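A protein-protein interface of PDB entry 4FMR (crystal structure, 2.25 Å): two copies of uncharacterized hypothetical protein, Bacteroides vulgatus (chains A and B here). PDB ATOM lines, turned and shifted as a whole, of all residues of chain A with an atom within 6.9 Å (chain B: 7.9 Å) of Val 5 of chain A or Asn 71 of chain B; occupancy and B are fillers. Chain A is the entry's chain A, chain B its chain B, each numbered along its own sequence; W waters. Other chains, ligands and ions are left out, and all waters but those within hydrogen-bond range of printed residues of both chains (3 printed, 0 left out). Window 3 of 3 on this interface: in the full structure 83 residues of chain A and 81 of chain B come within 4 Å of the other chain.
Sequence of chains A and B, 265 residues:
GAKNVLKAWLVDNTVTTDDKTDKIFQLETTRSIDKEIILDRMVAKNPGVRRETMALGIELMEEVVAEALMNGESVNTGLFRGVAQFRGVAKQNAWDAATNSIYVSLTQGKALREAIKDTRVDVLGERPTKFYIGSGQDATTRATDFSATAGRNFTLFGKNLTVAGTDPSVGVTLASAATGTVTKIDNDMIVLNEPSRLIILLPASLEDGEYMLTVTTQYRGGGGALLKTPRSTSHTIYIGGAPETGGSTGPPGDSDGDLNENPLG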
ATOM      1  N   LYS A   3      16.424   3.676  13.423  1.00  0.00           N
ATOM      2  CA  LYS A   3      17.383   4.716  13.052  1.00  0.00           C
ATOM      3  C   LYS A   3      18.474   4.916  14.146  1.00  0.00           C
ATOM      4  O   LYS A   3      19.676   4.926  13.830  1.00  0.00           O
ATOM      5  CB  LYS A   3      16.657   6.048  12.784  1.00  0.00           C
ATOM      6  N   ASN A   4      18.065   5.096  15.419  1.00  0.00           N
ATOM      7  CA  ASN A   4      19.043   5.328  16.484  1.00  0.00           C
ATOM      8  C   ASN A   4      19.467   4.018  17.135  1.00  0.00           C
ATOM      9  O   ASN A   4      18.687   3.071  17.172  1.00  0.00           O
ATOM     10  CB  ASN A   4      18.486   6.271  17.493  1.00  0.00           C
ATOM     11  CG  ASN A   4      18.121   7.598  16.880  1.00  0.00           C
ATOM     12  OD1 ASN A   4      18.980   8.340  16.361  1.00  0.00           O
ATOM     13  ND2 ASN A   4      16.836   7.915  16.932  1.00  0.00           N
ATOM     14  N   VAL A   5      20.737   3.941  17.578  1.00  0.00           N
ATOM     15  CA  VAL A   5      21.270   2.705  18.146  1.00  0.00           C
ATOM     16  C   VAL A   5      21.961   2.979  19.479  1.00  0.00           C
ATOM     17  O   VAL A   5      22.853   3.826  19.566  1.00  0.00           O
ATOM     18  CB  VAL A   5      22.235   1.953  17.173  1.00  0.00           C
ATOM     19  CG1 VAL A   5      22.683   0.623  17.765  1.00  0.00           C
ATOM     20  CG2 VAL A   5      21.598   1.734  15.808  1.00  0.00           C
ATOM     21  N   LEU A   6      21.516   2.257  20.521  1.00  0.00           N
ATOM     22  CA  LEU A   6      22.107   2.265  21.856  1.00  0.00           C
ATOM     23  C   LEU A   6      22.866   0.950  22.032  1.00  0.00           C
ATOM     24  O   LEU A   6      22.290  -0.126  21.836  1.00  0.00           O
ATOM     25  CB  LEU A   6      21.044   2.467  22.989  1.00  0.00           C
ATOM     26  CG  LEU A   6      20.212   3.749  23.009  1.00  0.00           C
ATOM     27  CD1 LEU A   6      19.163   3.689  24.071  1.00  0.00           C
ATOM     28  CD2 LEU A   6      21.058   4.963  23.218  1.00  0.00           C
ATOM     29  N   LYS A   7      24.169   1.036  22.339  1.00  0.00           N
ATOM     30  CA  LYS A   7      25.028  -0.136  22.570  1.00  0.00           C
ATOM     31  C   LYS A   7      24.993  -0.471  24.056  1.00  0.00           C
ATOM     32  O   LYS A   7      25.164   0.417  24.884  1.00  0.00           O
ATOM     33  CB  LYS A   7      26.462   0.135  22.072  1.00  0.00           C
ATOM     34  CG  LYS A   7      26.578   0.203  20.549  1.00  0.00           C
ATOM     35  CD  LYS A   7      27.953   0.699  20.104  1.00  0.00           C
ATOM     36  CE  LYS A   7      28.005   0.974  18.619  1.00  0.00           C
ATOM     37  NZ  LYS A   7      29.310   1.561  18.207  1.00  0.00           N
ATOM     38  N   LEU A  27      24.426   0.935  29.480  1.00  0.00           N
ATOM     39  CA  LEU A  27      24.872   1.703  28.319  1.00  0.00           C
ATOM     40  C   LEU A  27      26.392   1.720  28.239  1.00  0.00           C
ATOM     41  O   LEU A  27      27.048   1.973  29.247  1.00  0.00           O
ATOM     42  CB  LEU A  27      24.349   3.144  28.398  1.00  0.00           C
ATOM     43  CG  LEU A  27      24.446   3.958  27.120  1.00  0.00           C
ATOM     44  CD1 LEU A  27      23.419   3.491  26.081  1.00  0.00           C
ATOM     45  CD2 LEU A  27      24.240   5.447  27.416  1.00  0.00           C
ATOM     46  N   THR A  30      30.694   6.020  25.811  1.00  0.00           N
ATOM     47  CA  THR A  30      31.060   6.521  24.486  1.00  0.00           C
ATOM     48  C   THR A  30      31.574   7.972  24.553  1.00  0.00           C
ATOM     49  O   THR A  30      32.788   8.179  24.650  1.00  0.00           O
ATOM     50  CB  THR A  30      29.913   6.396  23.452  1.00  0.00           C
ATOM     51  OG1 THR A  30      28.730   6.988  23.966  1.00  0.00           O
ATOM     52  CG2 THR A  30      29.643   4.952  23.040  1.00  0.00           C
ATOM     53  N   ARG A  31      30.648   8.944  24.546  1.00  0.00           N
ATOM     54  CA  ARG A  31      30.884  10.374  24.424  1.00  0.00           C
ATOM     55  C   ARG A  31      29.986  11.229  25.284  1.00  0.00           C
ATOM     56  O   ARG A  31      28.845  10.871  25.564  1.00  0.00           O
ATOM     57  CB  ARG A  31      30.522  10.723  22.965  1.00  0.00           C
ATOM     58  CG  ARG A  31      31.478  11.531  22.176  1.00  0.00           C
ATOM     59  CD  ARG A  31      31.210  11.232  20.709  1.00  0.00           C
ATOM     60  NE  ARG A  31      31.445   9.815  20.382  1.00  0.00           N
ATOM     61  CZ  ARG A  31      30.496   8.931  20.068  1.00  0.00           C
ATOM     62  NH1 ARG A  31      29.224   9.310  19.982  1.00  0.00           N
ATOM     63  NH2 ARG A  31      30.817   7.673  19.802  1.00  0.00           N
ATOM     64  N   ASP A 118      11.973   5.175  17.845  1.00  0.00           N
ATOM     65  CA  ASP A 118      12.833   4.921  16.669  1.00  0.00           C
ATOM     66  C   ASP A 118      14.266   4.506  17.088  1.00  0.00           C
ATOM     67  O   ASP A 118      15.217   4.718  16.337  1.00  0.00           O
ATOM     68  CB  ASP A 118      12.903   6.171  15.750  1.00  0.00           C
ATOM     69  CG  ASP A 118      11.565   6.765  15.341  1.00  0.00           C
ATOM     70  OD1 ASP A 118      10.580   5.985  15.196  1.00  0.00           O
ATOM     71  OD2 ASP A 118      11.495   8.007  15.163  1.00  0.00           O
ATOM     72  N   THR A 119      14.411   3.917  18.273  1.00  0.00           N
ATOM     73  CA  THR A 119      15.719   3.518  18.796  1.00  0.00           C
ATOM     74  C   THR A 119      15.747   2.000  19.037  1.00  0.00           C
ATOM     75  O   THR A 119      14.783   1.424  19.546  1.00  0.00           O
ATOM     76  CB  THR A 119      16.017   4.334  20.069  1.00  0.00           C
ATOM     77  OG1 THR A 119      15.897   5.718  19.745  1.00  0.00           O
ATOM     78  CG2 THR A 119      17.408   4.078  20.648  1.00  0.00           C
ATOM     79  N   ARG A 120      16.856   1.360  18.644  1.00  0.00           N
ATOM     80  CA  ARG A 120      17.083  -0.053  18.888  1.00  0.00           C
ATOM     81  C   ARG A 120      18.299  -0.229  19.827  1.00  0.00           C
ATOM     82  O   ARG A 120      19.168   0.650  19.915  1.00  0.00           O
ATOM     83  CB  ARG A 120      17.234  -0.875  17.587  1.00  0.00           C
ATOM     84  CG  ARG A 120      18.383  -0.486  16.669  1.00  0.00           C
ATOM     85  CD  ARG A 120      18.510  -1.455  15.492  1.00  0.00           C
ATOM     86  NE  ARG A 120      19.786  -1.275  14.799  1.00  0.00           N
ATOM     87  CZ  ARG A 120      20.911  -1.910  15.117  1.00  0.00           C
ATOM     88  NH1 ARG A 120      20.922  -2.813  16.095  1.00  0.00           N
ATOM     89  NH2 ARG A 120      22.033  -1.657  14.454  1.00  0.00           N
ATOM     90  N   VAL A 121      18.335  -1.368  20.531  1.00  0.00           N
ATOM     91  CA  VAL A 121      19.396  -1.682  21.488  1.00  0.00           C
ATOM     92  C   VAL A 121      20.277  -2.776  20.896  1.00  0.00           C
ATOM     93  O   VAL A 121      19.790  -3.842  20.526  1.00  0.00           O
ATOM     94  CB  VAL A 121      18.821  -2.077  22.883  1.00  0.00           C
ATOM     95  CG1 VAL A 121      19.933  -2.461  23.869  1.00  0.00           C
ATOM     96  CG2 VAL A 121      17.949  -0.958  23.458  1.00  0.00           C
ATOM     97  N   ASP A 122      21.568  -2.464  20.742  1.00  0.00           N
ATOM     98  CA  ASP A 122      22.576  -3.400  20.261  1.00  0.00           C
ATOM     99  C   ASP A 122      23.267  -3.983  21.489  1.00  0.00           C
ATOM    100  O   ASP A 122      24.066  -3.308  22.130  1.00  0.00           O
ATOM    101  CB  ASP A 122      23.557  -2.694  19.298  1.00  0.00           C
ATOM    102  CG  ASP A 122      24.747  -3.498  18.799  1.00  0.00           C
ATOM    103  OD1 ASP A 122      24.802  -4.716  19.066  1.00  0.00           O
ATOM    104  OD2 ASP A 122      25.611  -2.910  18.119  1.00  0.00           O
ATOM    105  N   VAL B  64      18.986  17.839  17.744  1.00  0.00           N
ATOM    106  CA  VAL B  64      20.393  17.491  18.006  1.00  0.00           C
ATOM    107  C   VAL B  64      20.514  16.733  19.328  1.00  0.00           C
ATOM    108  O   VAL B  64      21.206  15.716  19.382  1.00  0.00           O
ATOM    109  CB  VAL B  64      21.274  18.773  18.001  1.00  0.00           C
ATOM    110  CG1 VAL B  64      22.662  18.530  18.617  1.00  0.00           C
ATOM    111  CG2 VAL B  64      21.373  19.350  16.595  1.00  0.00           C
ATOM    112  N   VAL B  65      19.875  17.249  20.383  1.00  0.00           N
ATOM    113  CA  VAL B  65      19.909  16.661  21.718  1.00  0.00           C
ATOM    114  C   VAL B  65      19.243  15.254  21.673  1.00  0.00           C
ATOM    115  O   VAL B  65      19.841  14.307  22.201  1.00  0.00           O
ATOM    116  CB  VAL B  65      19.264  17.595  22.793  1.00  0.00           C
ATOM    117  CG1 VAL B  65      19.017  16.845  24.105  1.00  0.00           C
ATOM    118  CG2 VAL B  65      20.143  18.827  23.048  1.00  0.00           C
ATOM    119  N   ALA B  66      18.054  15.127  21.026  1.00  0.00           N
ATOM    120  CA  ALA B  66      17.329  13.848  20.927  1.00  0.00           C
ATOM    121  C   ALA B  66      18.168  12.793  20.185  1.00  0.00           C
ATOM    122  O   ALA B  66      18.253  11.664  20.670  1.00  0.00           O
ATOM    123  CB  ALA B  66      15.964  14.021  20.240  1.00  0.00           C
ATOM    124  N   GLU B  67      18.823  13.176  19.063  1.00  0.00           N
ATOM    125  CA  GLU B  67      19.690  12.276  18.276  1.00  0.00           C
ATOM    126  C   GLU B  67      20.926  11.822  19.086  1.00  0.00           C
ATOM    127  O   GLU B  67      21.276  10.650  19.034  1.00  0.00           O
ATOM    128  CB  GLU B  67      20.155  12.929  16.957  1.00  0.00           C
ATOM    129  CG  GLU B  67      19.060  13.037  15.907  1.00  0.00           C
ATOM    130  CD  GLU B  67      19.311  13.992  14.747  1.00  0.00           C
ATOM    131  OE1 GLU B  67      20.459  14.468  14.582  1.00  0.00           O
ATOM    132  OE2 GLU B  67      18.341  14.276  14.007  1.00  0.00           O
ATOM    133  N   ALA B  68      21.552  12.750  19.833  1.00  0.00           N
ATOM    134  CA  ALA B  68      22.727  12.494  20.671  1.00  0.00           C
ATOM    135  C   ALA B  68      22.405  11.490  21.768  1.00  0.00           C
ATOM    136  O   ALA B  68      23.147  10.546  21.957  1.00  0.00           O
ATOM    137  CB  ALA B  68      23.227  13.797  21.279  1.00  0.00           C
ATOM    138  N   LEU B  69      21.275  11.676  22.460  1.00  0.00           N
ATOM    139  CA  LEU B  69      20.817  10.796  23.528  1.00  0.00           C
ATOM    140  C   LEU B  69      20.493   9.399  23.037  1.00  0.00           C
ATOM    141  O   LEU B  69      20.848   8.406  23.696  1.00  0.00           O
ATOM    142  CB  LEU B  69      19.571  11.395  24.187  1.00  0.00           C
ATOM    143  CG  LEU B  69      19.824  12.575  25.100  1.00  0.00           C
ATOM    144  CD1 LEU B  69      18.555  13.312  25.379  1.00  0.00           C
ATOM    145  CD2 LEU B  69      20.561  12.149  26.379  1.00  0.00           C
ATOM    146  N   MET B  70      19.836   9.327  21.866  1.00  0.00           N
ATOM    147  CA  MET B  70      19.380   8.078  21.258  1.00  0.00           C
ATOM    148  C   MET B  70      20.530   7.343  20.568  1.00  0.00           C
ATOM    149  O   MET B  70      20.358   6.193  20.188  1.00  0.00           O
ATOM    150  CB  MET B  70      18.202   8.344  20.298  1.00  0.00           C
ATOM    151  CG  MET B  70      16.908   8.696  21.043  1.00  0.00           C
ATOM    152  SD  MET B  70      16.497   7.336  22.397  1.00  0.00           S
ATOM    153  CE  MET B  70      16.894   8.299  24.008  1.00  0.00           C
ATOM    154  N   ASN B  71      21.721   7.949  20.518  1.00  0.00           N
ATOM    155  CA  ASN B  71      22.904   7.287  20.016  1.00  0.00           C
ATOM    156  C   ASN B  71      23.918   7.126  21.173  1.00  0.00           C
ATOM    157  O   ASN B  71      25.079   6.823  20.953  1.00  0.00           O
ATOM    158  CB  ASN B  71      23.476   7.987  18.773  1.00  0.00           C
ATOM    159  CG  ASN B  71      22.586   7.661  17.581  1.00  0.00           C
ATOM    160  OD1 ASN B  71      22.660   6.558  17.002  1.00  0.00           O
ATOM    161  ND2 ASN B  71      21.583   8.517  17.323  1.00  0.00           N
ATOM    162  N   GLY B  72      23.417   7.203  22.400  1.00  0.00           N
ATOM    163  CA  GLY B  72      24.158   6.846  23.601  1.00  0.00           C
ATOM    164  C   GLY B  72      25.141   7.825  24.173  1.00  0.00           C
ATOM    165  O   GLY B  72      25.968   7.447  24.999  1.00  0.00           O
ATOM    166  N   GLU B  73      25.035   9.087  23.769  1.00  0.00           N
ATOM    167  CA  GLU B  73      25.882  10.119  24.316  1.00  0.00           C
ATOM    168  C   GLU B  73      25.207  10.742  25.547  1.00  0.00           C
ATOM    169  O   GLU B  73      23.976  10.781  25.646  1.00  0.00           O
ATOM    170  CB  GLU B  73      26.175  11.186  23.257  1.00  0.00           C
ATOM    171  CG  GLU B  73      26.851  10.679  21.986  1.00  0.00           C
ATOM    172  CD  GLU B  73      26.952  11.700  20.858  1.00  0.00           C
ATOM    173  OE1 GLU B  73      26.137  12.645  20.849  1.00  0.00           O
ATOM    174  OE2 GLU B  73      27.834  11.557  19.981  1.00  0.00           O
ATOM    175  N   SER B  74      26.008  11.179  26.502  1.00  0.00           N
ATOM    176  CA  SER B  74      25.477  11.950  27.612  1.00  0.00           C
ATOM    177  C   SER B  74      25.432  13.398  27.118  1.00  0.00           C
ATOM    178  O   SER B  74      26.327  13.833  26.374  1.00  0.00           O
ATOM    179  CB  SER B  74      26.290  11.764  28.891  1.00  0.00           C
ATOM    180  OG  SER B  74      27.654  12.017  28.640  1.00  0.00           O
ATOM    181  N   ALA B  84      20.641   8.184  28.279  1.00  0.00           N
ATOM    182  CA  ALA B  84      19.716   7.053  28.112  1.00  0.00           C
ATOM    183  C   ALA B  84      19.941   6.024  29.235  1.00  0.00           C
ATOM    184  O   ALA B  84      21.092   5.765  29.649  1.00  0.00           O
ATOM    185  CB  ALA B  84      19.930   6.385  26.747  1.00  0.00           C
ATOM    186  N   PHE B  86      18.093   2.053  30.866  1.00  0.00           N
ATOM    187  CA  PHE B  86      17.297   0.854  30.555  1.00  0.00           C
ATOM    188  C   PHE B  86      16.465   0.375  31.742  1.00  0.00           C
ATOM    189  O   PHE B  86      16.879   0.505  32.894  1.00  0.00           O
ATOM    190  CB  PHE B  86      18.226  -0.296  30.101  1.00  0.00           C
ATOM    191  CG  PHE B  86      19.099   0.089  28.927  1.00  0.00           C
ATOM    192  CD1 PHE B  86      18.537   0.395  27.686  1.00  0.00           C
ATOM    193  CD2 PHE B  86      20.485   0.191  29.068  1.00  0.00           C
ATOM    194  CE1 PHE B  86      19.342   0.758  26.604  1.00  0.00           C
ATOM    195  CE2 PHE B  86      21.288   0.537  27.977  1.00  0.00           C
ATOM    196  CZ  PHE B  86      20.710   0.821  26.753  1.00  0.00           C
ATOM    197  N   ILE B 102      13.535   1.873  27.195  1.00  0.00           N
ATOM    198  CA  ILE B 102      14.473   2.971  27.225  1.00  0.00           C
ATOM    199  C   ILE B 102      13.754   4.188  27.784  1.00  0.00           C
ATOM    200  O   ILE B 102      12.575   4.401  27.505  1.00  0.00           O
ATOM    201  CB  ILE B 102      15.051   3.260  25.804  1.00  0.00           C
ATOM    202  CG1 ILE B 102      15.590   1.996  25.094  1.00  0.00           C
ATOM    203  CG2 ILE B 102      16.079   4.424  25.810  1.00  0.00           C
ATOM    204  CD1 ILE B 102      15.813   2.190  23.536  1.00  0.00           C
HETATM  205  O   HOH W   1      28.335   7.758  27.550  1.00  0.00           O
HETATM  206  O   HOH W   2      26.868   4.895  24.723  1.00  0.00           O
HETATM  207  O   HOH W   3      22.379   6.412  14.013  1.00  0.00           O
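The side-chain hydroxyl (OG1) of Thr 30 of chain A sits at hydrogen-bond distance from the backbone carbonyl oxygen (O) of Gly 72 of chain B, at 3.0 Å. OD1 of Asn 4 of chain A is in hydrogen-bond range of ND2 of Asn 71 of chain B (2.8 Å). N of Val 5 of chain A sits at hydrogen-bond distance from OD1 of Asn 71 of chain B (3.3 Å). The backbone carbonyl oxygen (O) of Arg 31 of chain A sits at hydrogen-bond distance from the backbone NH (N) of Ser 74 of chain B, at 3.0 Å. The side-chain sulfur (SD) of Met 70 of chain B sits at hydrogen-bond distance from the side-chain hydroxyl (OG1) of Thr 119 of chain A. NH1 of Arg 31 of chain A is in salt-bridge range of OE2 of Glu 73 of chain B (2.6 Å). The backbone NH (N) of Val 5 of chain A is in hydrogen-bond range of the backbone carbonyl oxygen (O) of Met 70 of chain B (3.5 Å).
N of Arg 120 of chain A is in hydrogen-bond range of O of Asn 4 of chain A, 2.9 Å away. O of Glu 67 of chain B is in hydrogen-bond range of ND2 of Asn 71 of chain B. O of Asp 118 of chain A is in hydrogen-bond range of N of Asn 4 of chain A (3.0 Å). N of Glu 73 of chain B sits at hydrogen-bond distance from O of Ala 68 of chain B (3.0 Å). O of Arg 120 of chain A lies within hydrogen-bond range of N of Leu 6 of chain A, 2.9 Å away. O of Leu 6 of chain A lies within hydrogen-bond range of N of Asp 122 of chain A.
Hydrophobic or aromatic side chains of chain A within 4 Å of the printed part of chain B: Leu 6, Leu 27 and Val 121. Printed residues of chain B that touch a printed residue of chain A: Leu 69, Met 70, Asn 71, Gly 72, Glu 73, Ser 74, Ala 84, Phe 86 and Ile 102. Hydrophobic or aromatic side chains of chain B within 4 Å of the printed part of chain A: Met 70, Ala 84, Phe 86 and Ile 102. Among the printed residues, 20 pairs touch across the chains. Among the printed residues, Asp or Glu carboxylates within 4 Å of a Lys or Arg side-chain nitrogen of the other chain: Arg 31 of chain A with Glu 73 of chain B (2.6 Å).
Asn 71 of chain B touches two residues of chain A. Of the printed residues of chain B, Thr 119 of chain A touches Met 70 and Ile 102. Of the printed residues of chain B, Leu 6 of chain A touches Leu 69, Met 70, Gly 72, Ala 84, Phe 86 and Ile 102. Printed residues of chain B within 4 Å of Thr 30 of chain A: Gly 72 (3.0 Å). Of the printed residues of chain B, Leu 27 of chain A touches Gly 72 (3.6 Å), Ala 84 (3.9 Å) and Phe 86 (3.5 Å). Val 65 of chain B touches none of the printed residues of chain A. The nearest residue of chain B that does not touch Val 5 of chain A is Gly 72 of chain B (4.4 Å). The nearest printed residue of chain B that does not touch Asn 4 of chain A is Glu 67 of chain B (4.2 Å).
O of Leu 69 of chain B touches CD2 of Leu 6 of chain A, at 3.5 Å. Leu 6 of chain A touches Met 70 of chain B (CD2 to O, 3.3 Å). Gly 72 of chain B touches Leu 6 of chain A. Phe 86 of chain B touches Leu 6 of chain A (CE1 to CD1, 3.9 Å). CG2 of Ile 102 of chain B touches CD1 of Leu 6 of chain A (3.6 Å). CD2 of Leu 27 of chain A touches O of Gly 72 of chain B (3.6 Å). CD2 of Leu 27 of chain A touches O of Ala 84 of chain B (3.9 Å). CE2 of Phe 86 of chain B touches N of Leu 27 of chain A, 3.5 Å away. Phe 86 of chain B touches Val 121 of chain A. CD1 of Ile 102 of chain B touches CG2 of Val 121 of chain A (3.8 Å).
Water W2 bridges O of Gly 72 of chain B (2.7 Å) and OG1 of Thr 30 of chain A (2.9 Å). Water W3 lies within hydrogen-bond range of the side-chain amide oxygen (OD1) of Asn 71 of chain B (3.0 Å) and the backbone carbonyl oxygen (O) of Lys 3 of chain A (3.1 Å). Water W1 lies within hydrogen-bond range of N of Thr 30 of chain A (3.4 Å) and O of Gly 72 of chain B (3.5 Å).
No position is printed for both chains. Of the 20 pairs that touch across the chains among the printed residues, none has its exchanged pair printed and touching as well.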
